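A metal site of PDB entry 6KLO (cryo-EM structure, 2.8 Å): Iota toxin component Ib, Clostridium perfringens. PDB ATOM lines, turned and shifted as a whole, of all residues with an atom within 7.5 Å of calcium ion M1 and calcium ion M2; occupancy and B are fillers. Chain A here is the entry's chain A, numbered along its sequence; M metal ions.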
ATOM      1  N   LEU A   9      -2.535 -29.743 -28.878  1.00  0.00           N
ATOM      2  CA  LEU A   9      -1.446 -29.086 -29.574  1.00  0.00           C
ATOM      3  C   LEU A   9      -0.689 -28.159 -28.625  1.00  0.00           C
ATOM      4  O   LEU A   9      -1.289 -27.506 -27.780  1.00  0.00           O
ATOM      5  CB  LEU A   9      -1.977 -28.291 -30.769  1.00  0.00           C
ATOM      6  CG  LEU A   9      -0.995 -27.420 -31.552  1.00  0.00           C
ATOM      7  CD1 LEU A   9       0.067 -28.277 -32.214  1.00  0.00           C
ATOM      8  CD2 LEU A   9      -1.739 -26.594 -32.575  1.00  0.00           C
ATOM      9  N   ASP A  10       0.635 -28.114 -28.785  1.00  0.00           N
ATOM     10  CA  ASP A  10       1.510 -27.245 -27.993  1.00  0.00           C
ATOM     11  C   ASP A  10       2.414 -26.509 -28.987  1.00  0.00           C
ATOM     12  O   ASP A  10       3.372 -27.095 -29.499  1.00  0.00           O
ATOM     13  CB  ASP A  10       2.315 -28.057 -26.986  1.00  0.00           C
ATOM     14  CG  ASP A  10       3.024 -27.189 -25.981  1.00  0.00           C
ATOM     15  OD1 ASP A  10       2.630 -26.015 -25.815  1.00  0.00           O
ATOM     16  OD2 ASP A  10       3.976 -27.688 -25.338  1.00  0.00           O
ATOM     17  N   THR A  11       2.104 -25.243 -29.249  1.00  0.00           N
ATOM     18  CA  THR A  11       2.801 -24.518 -30.301  1.00  0.00           C
ATOM     19  C   THR A  11       4.177 -24.055 -29.835  1.00  0.00           C
ATOM     20  O   THR A  11       5.168 -24.168 -30.572  1.00  0.00           O
ATOM     21  CB  THR A  11       1.963 -23.331 -30.765  1.00  0.00           C
ATOM     22  OG1 THR A  11       0.724 -23.803 -31.294  1.00  0.00           O
ATOM     23  CG2 THR A  11       2.700 -22.567 -31.849  1.00  0.00           C
ATOM     24  N   ASP A  12       4.269 -23.531 -28.611  1.00  0.00           N
ATOM     25  CA  ASP A  12       5.530 -23.006 -28.112  1.00  0.00           C
ATOM     26  C   ASP A  12       6.369 -24.054 -27.403  1.00  0.00           C
ATOM     27  O   ASP A  12       7.476 -23.725 -26.954  1.00  0.00           O
ATOM     28  CB  ASP A  12       5.269 -21.837 -27.162  1.00  0.00           C
ATOM     29  CG  ASP A  12       4.171 -22.120 -26.179  1.00  0.00           C
ATOM     30  OD1 ASP A  12       3.529 -23.182 -26.305  1.00  0.00           O
ATOM     31  OD2 ASP A  12       3.941 -21.292 -25.287  1.00  0.00           O
ATOM     32  N   ASN A  13       5.889 -25.295 -27.295  1.00  0.00           N
ATOM     33  CA  ASN A  13       6.618 -26.397 -26.659  1.00  0.00           C
ATOM     34  C   ASN A  13       7.080 -26.026 -25.257  1.00  0.00           C
ATOM     35  O   ASN A  13       8.271 -25.972 -24.945  1.00  0.00           O
ATOM     36  CB  ASN A  13       7.801 -26.837 -27.520  1.00  0.00           C
ATOM     37  CG  ASN A  13       7.435 -27.019 -28.987  1.00  0.00           C
ATOM     38  OD1 ASN A  13       6.655 -27.901 -29.328  1.00  0.00           O
ATOM     39  ND2 ASN A  13       7.990 -26.182 -29.840  1.00  0.00           N
ATOM     40  N   ASP A  14       6.104 -25.746 -24.383  1.00  0.00           N
ATOM     41  CA  ASP A  14       6.374 -25.545 -22.966  1.00  0.00           C
ATOM     42  C   ASP A  14       5.564 -26.500 -22.098  1.00  0.00           C
ATOM     43  O   ASP A  14       5.458 -26.288 -20.895  1.00  0.00           O
ATOM     44  CB  ASP A  14       6.101 -24.097 -22.552  1.00  0.00           C
ATOM     45  CG  ASP A  14       4.696 -23.649 -22.886  1.00  0.00           C
ATOM     46  OD1 ASP A  14       3.978 -24.381 -23.597  1.00  0.00           O
ATOM     47  OD2 ASP A  14       4.310 -22.548 -22.451  1.00  0.00           O
ATOM     48  N   ASN A  15       5.002 -27.554 -22.696  1.00  0.00           N
ATOM     49  CA  ASN A  15       4.273 -28.600 -21.997  1.00  0.00           C
ATOM     50  C   ASN A  15       2.949 -28.112 -21.417  1.00  0.00           C
ATOM     51  O   ASN A  15       2.479 -28.641 -20.406  1.00  0.00           O
ATOM     52  CB  ASN A  15       5.126 -29.248 -20.901  1.00  0.00           C
ATOM     53  CG  ASN A  15       6.520 -29.597 -21.377  1.00  0.00           C
ATOM     54  OD1 ASN A  15       6.712 -30.003 -22.524  1.00  0.00           O
ATOM     55  ND2 ASN A  15       7.503 -29.440 -20.496  1.00  0.00           N
ATOM     56  N   ILE A  16       2.346 -27.106 -22.037  1.00  0.00           N
ATOM     57  CA  ILE A  16       0.990 -26.686 -21.708  1.00  0.00           C
ATOM     58  C   ILE A  16       0.260 -26.481 -23.030  1.00  0.00           C
ATOM     59  O   ILE A  16       0.682 -25.652 -23.845  1.00  0.00           O
ATOM     60  CB  ILE A  16       0.941 -25.400 -20.864  1.00  0.00           C
ATOM     61  CG1 ILE A  16       1.956 -25.453 -19.727  1.00  0.00           C
ATOM     62  CG2 ILE A  16      -0.448 -25.200 -20.294  1.00  0.00           C
ATOM     63  CD1 ILE A  16       2.117 -24.146 -19.017  1.00  0.00           C
ATOM     64  N   PRO A  17      -0.822 -27.198 -23.296  1.00  0.00           N
ATOM     65  CA  PRO A  17      -1.520 -27.051 -24.579  1.00  0.00           C
ATOM     66  C   PRO A  17      -2.048 -25.648 -24.792  1.00  0.00           C
ATOM     67  O   PRO A  17      -2.261 -24.876 -23.844  1.00  0.00           O
ATOM     68  CB  PRO A  17      -2.667 -28.062 -24.487  1.00  0.00           C
ATOM     69  CG  PRO A  17      -2.215 -29.040 -23.462  1.00  0.00           C
ATOM     70  CD  PRO A  17      -1.414 -28.262 -22.480  1.00  0.00           C
ATOM     71  N   ASP A  18      -2.269 -25.300 -26.062  1.00  0.00           N
ATOM     72  CA  ASP A  18      -2.753 -23.973 -26.413  1.00  0.00           C
ATOM     73  C   ASP A  18      -4.114 -23.690 -25.805  1.00  0.00           C
ATOM     74  O   ASP A  18      -4.361 -22.593 -25.281  1.00  0.00           O
ATOM     75  CB  ASP A  18      -2.817 -23.810 -27.923  1.00  0.00           C
ATOM     76  CG  ASP A  18      -1.459 -23.940 -28.585  1.00  0.00           C
ATOM     77  OD1 ASP A  18      -0.490 -24.275 -27.883  1.00  0.00           O
ATOM     78  OD2 ASP A  18      -1.366 -23.703 -29.808  1.00  0.00           O
ATOM     79  N   ALA A  19      -5.030 -24.650 -25.882  1.00  0.00           N
ATOM     80  CA  ALA A  19      -6.369 -24.450 -25.337  1.00  0.00           C
ATOM     81  C   ALA A  19      -6.319 -24.158 -23.855  1.00  0.00           C
ATOM     82  O   ALA A  19      -7.037 -23.272 -23.365  1.00  0.00           O
ATOM     83  CB  ALA A  19      -7.237 -25.680 -25.613  1.00  0.00           C
ATOM     84  N   GLU A  21      -3.719 -22.871 -22.139  1.00  0.00           N
ATOM     85  CA  GLU A  21      -3.078 -21.580 -21.891  1.00  0.00           C
ATOM     86  C   GLU A  21      -3.978 -20.409 -22.252  1.00  0.00           C
ATOM     87  O   GLU A  21      -3.839 -19.330 -21.683  1.00  0.00           O
ATOM     88  CB  GLU A  21      -1.756 -21.503 -22.661  1.00  0.00           C
ATOM     89  CG  GLU A  21      -0.582 -21.917 -21.801  1.00  0.00           C
ATOM     90  CD  GLU A  21       0.744 -21.627 -22.449  1.00  0.00           C
ATOM     91  OE1 GLU A  21       0.796 -21.495 -23.673  1.00  0.00           O
ATOM     92  OE2 GLU A  21       1.743 -21.493 -21.713  1.00  0.00           O
ATOM     93  N   TYR A  25      -5.907 -23.055 -16.830  1.00  0.00           N
ATOM     94  CA  TYR A  25      -5.376 -24.354 -16.445  1.00  0.00           C
ATOM     95  C   TYR A  25      -4.845 -24.269 -15.024  1.00  0.00           C
ATOM     96  O   TYR A  25      -4.701 -23.183 -14.451  1.00  0.00           O
ATOM     97  CB  TYR A  25      -4.284 -24.813 -17.398  1.00  0.00           C
ATOM     98  CG  TYR A  25      -3.045 -23.943 -17.385  1.00  0.00           C
ATOM     99  CD1 TYR A  25      -2.953 -22.824 -18.193  1.00  0.00           C
ATOM    100  CD2 TYR A  25      -1.967 -24.243 -16.572  1.00  0.00           C
ATOM    101  CE1 TYR A  25      -1.836 -22.029 -18.191  1.00  0.00           C
ATOM    102  CE2 TYR A  25      -0.848 -23.453 -16.563  1.00  0.00           C
ATOM    103  CZ  TYR A  25      -0.782 -22.352 -17.377  1.00  0.00           C
ATOM    104  OH  TYR A  25       0.335 -21.557 -17.375  1.00  0.00           O
ATOM    105  N   SER A  49      -1.909 -17.850 -19.959  1.00  0.00           N
ATOM    106  CA  SER A  49      -0.612 -17.538 -20.523  1.00  0.00           C
ATOM    107  C   SER A  49      -0.750 -17.334 -22.023  1.00  0.00           C
ATOM    108  O   SER A  49      -1.784 -17.620 -22.621  1.00  0.00           O
ATOM    109  CB  SER A  49       0.404 -18.639 -20.240  1.00  0.00           C
ATOM    110  OG  SER A  49       0.617 -18.794 -18.847  1.00  0.00           O
ATOM    111  N   SER A  50       0.317 -16.832 -22.624  1.00  0.00           N
ATOM    112  CA  SER A  50       0.400 -16.749 -24.075  1.00  0.00           C
ATOM    113  C   SER A  50       0.725 -18.123 -24.637  1.00  0.00           C
ATOM    114  O   SER A  50       1.694 -18.768 -24.225  1.00  0.00           O
ATOM    115  CB  SER A  50       1.467 -15.746 -24.488  1.00  0.00           C
ATOM    116  OG  SER A  50       1.392 -15.469 -25.879  1.00  0.00           O
ATOM    117  N   TYR A  51      -0.083 -18.582 -25.583  1.00  0.00           N
ATOM    118  CA  TYR A  51       0.183 -19.880 -26.202  1.00  0.00           C
ATOM    119  C   TYR A  51       1.207 -19.789 -27.314  1.00  0.00           C
ATOM    120  O   TYR A  51       1.485 -20.806 -27.963  1.00  0.00           O
ATOM    121  CB  TYR A  51      -1.121 -20.503 -26.709  1.00  0.00           C
ATOM    122  CG  TYR A  51      -1.727 -19.832 -27.923  1.00  0.00           C
ATOM    123  CD1 TYR A  51      -2.600 -18.769 -27.782  1.00  0.00           C
ATOM    124  CD2 TYR A  51      -1.432 -20.283 -29.200  1.00  0.00           C
ATOM    125  CE1 TYR A  51      -3.151 -18.169 -28.884  1.00  0.00           C
ATOM    126  CE2 TYR A  51      -1.984 -19.683 -30.303  1.00  0.00           C
ATOM    127  CZ  TYR A  51      -2.851 -18.637 -30.138  1.00  0.00           C
ATOM    128  OH  TYR A  51      -3.398 -18.025 -31.245  1.00  0.00           O
ATOM    129  N   LEU A  52       1.780 -18.614 -27.551  1.00  0.00           N
ATOM    130  CA  LEU A  52       2.843 -18.428 -28.531  1.00  0.00           C
ATOM    131  C   LEU A  52       4.162 -18.010 -27.885  1.00  0.00           C
ATOM    132  O   LEU A  52       5.110 -17.683 -28.603  1.00  0.00           O
ATOM    133  CB  LEU A  52       2.426 -17.388 -29.571  1.00  0.00           C
ATOM    134  CG  LEU A  52       1.336 -17.776 -30.562  1.00  0.00           C
ATOM    135  CD1 LEU A  52       1.113 -16.645 -31.546  1.00  0.00           C
ATOM    136  CD2 LEU A  52       1.691 -19.052 -31.286  1.00  0.00           C
ATOM    137  N   GLU A  53       4.233 -18.014 -26.564  1.00  0.00           N
ATOM    138  CA  GLU A  53       5.438 -17.643 -25.836  1.00  0.00           C
ATOM    139  C   GLU A  53       5.698 -18.643 -24.732  1.00  0.00           C
ATOM    140  O   GLU A  53       4.780 -18.988 -23.971  1.00  0.00           O
ATOM    141  CB  GLU A  53       5.329 -16.242 -25.233  1.00  0.00           C
ATOM    142  CG  GLU A  53       5.573 -15.115 -26.220  1.00  0.00           C
ATOM    143  CD  GLU A  53       7.049 -14.867 -26.449  1.00  0.00           C
ATOM    144  OE1 GLU A  53       7.868 -15.334 -25.628  1.00  0.00           O
ATOM    145  OE2 GLU A  53       7.386 -14.203 -27.458  1.00  0.00           O
ATOM    146  N   SER A  54       6.939 -19.119 -24.626  1.00  0.00           N
ATOM    147  CA  SER A  54       7.312 -19.980 -23.514  1.00  0.00           C
ATOM    148  C   SER A  54       7.539 -19.175 -22.239  1.00  0.00           C
ATOM    149  O   SER A  54       7.392 -19.719 -21.142  1.00  0.00           O
ATOM    150  CB  SER A  54       8.564 -20.767 -23.851  1.00  0.00           C
ATOM    151  OG  SER A  54       8.330 -21.659 -24.913  1.00  0.00           O
ATOM    152  N   ASN A  55       7.901 -17.909 -22.375  1.00  0.00           N
ATOM    153  CA  ASN A  55       8.192 -17.022 -21.256  1.00  0.00           C
ATOM    154  C   ASN A  55       7.289 -15.807 -21.425  1.00  0.00           C
ATOM    155  O   ASN A  55       7.686 -14.804 -22.026  1.00  0.00           O
ATOM    156  CB  ASN A  55       9.662 -16.631 -21.211  1.00  0.00           C
ATOM    157  CG  ASN A  55      10.565 -17.806 -20.903  1.00  0.00           C
ATOM    158  OD1 ASN A  55      10.916 -18.033 -19.754  1.00  0.00           O
ATOM    159  ND2 ASN A  55      10.963 -18.522 -21.930  1.00  0.00           N
ATOM    160  N   THR A  56       6.070 -15.910 -20.909  1.00  0.00           N
ATOM    161  CA  THR A  56       5.111 -14.827 -21.081  1.00  0.00           C
ATOM    162  C   THR A  56       5.556 -13.554 -20.376  1.00  0.00           C
ATOM    163  O   THR A  56       5.476 -12.461 -20.937  1.00  0.00           O
ATOM    164  CB  THR A  56       3.736 -15.263 -20.585  1.00  0.00           C
ATOM    165  OG1 THR A  56       3.238 -16.322 -21.413  1.00  0.00           O
ATOM    166  CG2 THR A  56       2.756 -14.110 -20.617  1.00  0.00           C
ATOM    167  N   THR A  62      10.025 -20.522 -17.574  1.00  0.00           N
ATOM    168  CA  THR A  62       8.923 -20.712 -18.499  1.00  0.00           C
ATOM    169  C   THR A  62       7.587 -20.715 -17.773  1.00  0.00           C
ATOM    170  O   THR A  62       7.519 -20.714 -16.540  1.00  0.00           O
ATOM    171  CB  THR A  62       9.088 -22.007 -19.291  1.00  0.00           C
ATOM    172  OG1 THR A  62       8.741 -23.121 -18.468  1.00  0.00           O
ATOM    173  CG2 THR A  62      10.513 -22.177 -19.761  1.00  0.00           C
ATOM    174  N   ASP A  63       6.511 -20.694 -18.557  1.00  0.00           N
ATOM    175  CA  ASP A  63       5.162 -20.722 -17.982  1.00  0.00           C
ATOM    176  C   ASP A  63       4.951 -21.970 -17.137  1.00  0.00           C
ATOM    177  O   ASP A  63       4.370 -21.909 -16.050  1.00  0.00           O
ATOM    178  CB  ASP A  63       4.121 -20.640 -19.079  1.00  0.00           C
ATOM    179  CG  ASP A  63       4.254 -19.398 -19.923  1.00  0.00           C
ATOM    180  OD1 ASP A  63       4.939 -18.456 -19.493  1.00  0.00           O
ATOM    181  OD2 ASP A  63       3.672 -19.351 -21.030  1.00  0.00           O
ATOM    182  N   TYR A  64       5.432 -23.119 -17.629  1.00  0.00           N
ATOM    183  CA  TYR A  64       5.233 -24.363 -16.895  1.00  0.00           C
ATOM    184  C   TYR A  64       6.110 -24.414 -15.650  1.00  0.00           C
ATOM    185  O   TYR A  64       5.663 -24.873 -14.596  1.00  0.00           O
ATOM    186  CB  TYR A  64       5.514 -25.564 -17.785  1.00  0.00           C
ATOM    187  CG  TYR A  64       5.446 -26.866 -17.037  1.00  0.00           C
ATOM    188  CD1 TYR A  64       4.225 -27.418 -16.695  1.00  0.00           C
ATOM    189  CD2 TYR A  64       6.592 -27.524 -16.637  1.00  0.00           C
ATOM    190  CE1 TYR A  64       4.153 -28.596 -15.995  1.00  0.00           C
ATOM    191  CE2 TYR A  64       6.534 -28.698 -15.939  1.00  0.00           C
ATOM    192  CZ  TYR A  64       5.307 -29.233 -15.621  1.00  0.00           C
ATOM    193  OH  TYR A  64       5.230 -30.418 -14.925  1.00  0.00           O
ATOM    194  N   PRO A  82       2.184 -17.064 -14.182  1.00  0.00           N
ATOM    195  CA  PRO A  82       2.885 -16.763 -15.442  1.00  0.00           C
ATOM    196  C   PRO A  82       2.775 -15.323 -15.903  1.00  0.00           C
ATOM    197  O   PRO A  82       3.476 -14.949 -16.841  1.00  0.00           O
ATOM    198  CB  PRO A  82       2.226 -17.714 -16.443  1.00  0.00           C
ATOM    199  CG  PRO A  82       1.694 -18.817 -15.619  1.00  0.00           C
ATOM    200  CD  PRO A  82       1.270 -18.213 -14.328  1.00  0.00           C
HETATM  201 CA    CA M   1       1.979 -23.894 -24.731  1.00  0.00          CA
HETATM  202 CA    CA M   2       3.136 -20.409 -23.252  1.00  0.00          CA
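OG1 of Thr 56 lies within hydrogen-bond range of N of Ser 50 (3.2 Å). The side-chain carboxylate (OD1) of Asp 63 is in hydrogen-bond range of the backbone NH (N) of Thr 56, 3.1 Å away. The backbone carbonyl oxygen of Asp 12 sits at hydrogen-bond distance from the side-chain hydroxyl of Ser 54, 3.0 Å away. N of Asn 15 is in hydrogen-bond range of OD2 of Asp 10, at 2.8 Å. The backbone carbonyl oxygen of Ser 54 lies within hydrogen-bond range of the backbone NH of Asp 63 (2.9 Å). The backbone NH (N) of Ser 49 lies within hydrogen-bond range of the backbone carbonyl oxygen (O) of Glu 21. The backbone carbonyl oxygen of Asp 10 lies close to the side-chain amide oxygen of Asn 13 (3.4 Å).
Of the 25 residues printed, 5 come within 4 Å of calcium ion M1.
Of the 25 residues printed, 6 come within 4 Å of calcium ion M2. The nearest printed residue that does not touch calcium ion M2 is Ser 54 (4.2 Å).
Calcium ion M1 is bound by OD1 of Asp 12 (2.3 Å), OD1 of Asp 14 (2.3 Å), O of Ile 16 (2.4 Å), OD1 of Asp 10 (2.5 Å) and OE1 of Glu 21 (2.9 Å).
O of Glu 53 binds calcium ion M2 (2.3 Å). OE2 of Glu 21 binds calcium ion M2, 2.3 Å away. The side-chain carboxylate (OD2) of Asp 12 binds calcium ion M2. O of Ser 50 is bound to calcium ion M2. OD2 of Asp 63 binds calcium ion M2 (2.5 Å). Calcium ion M2 is bound by OD2 of Asp 14 (2.6 Å). OE1 of Glu 21 is bound to calcium ion M2 (2.6 Å).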
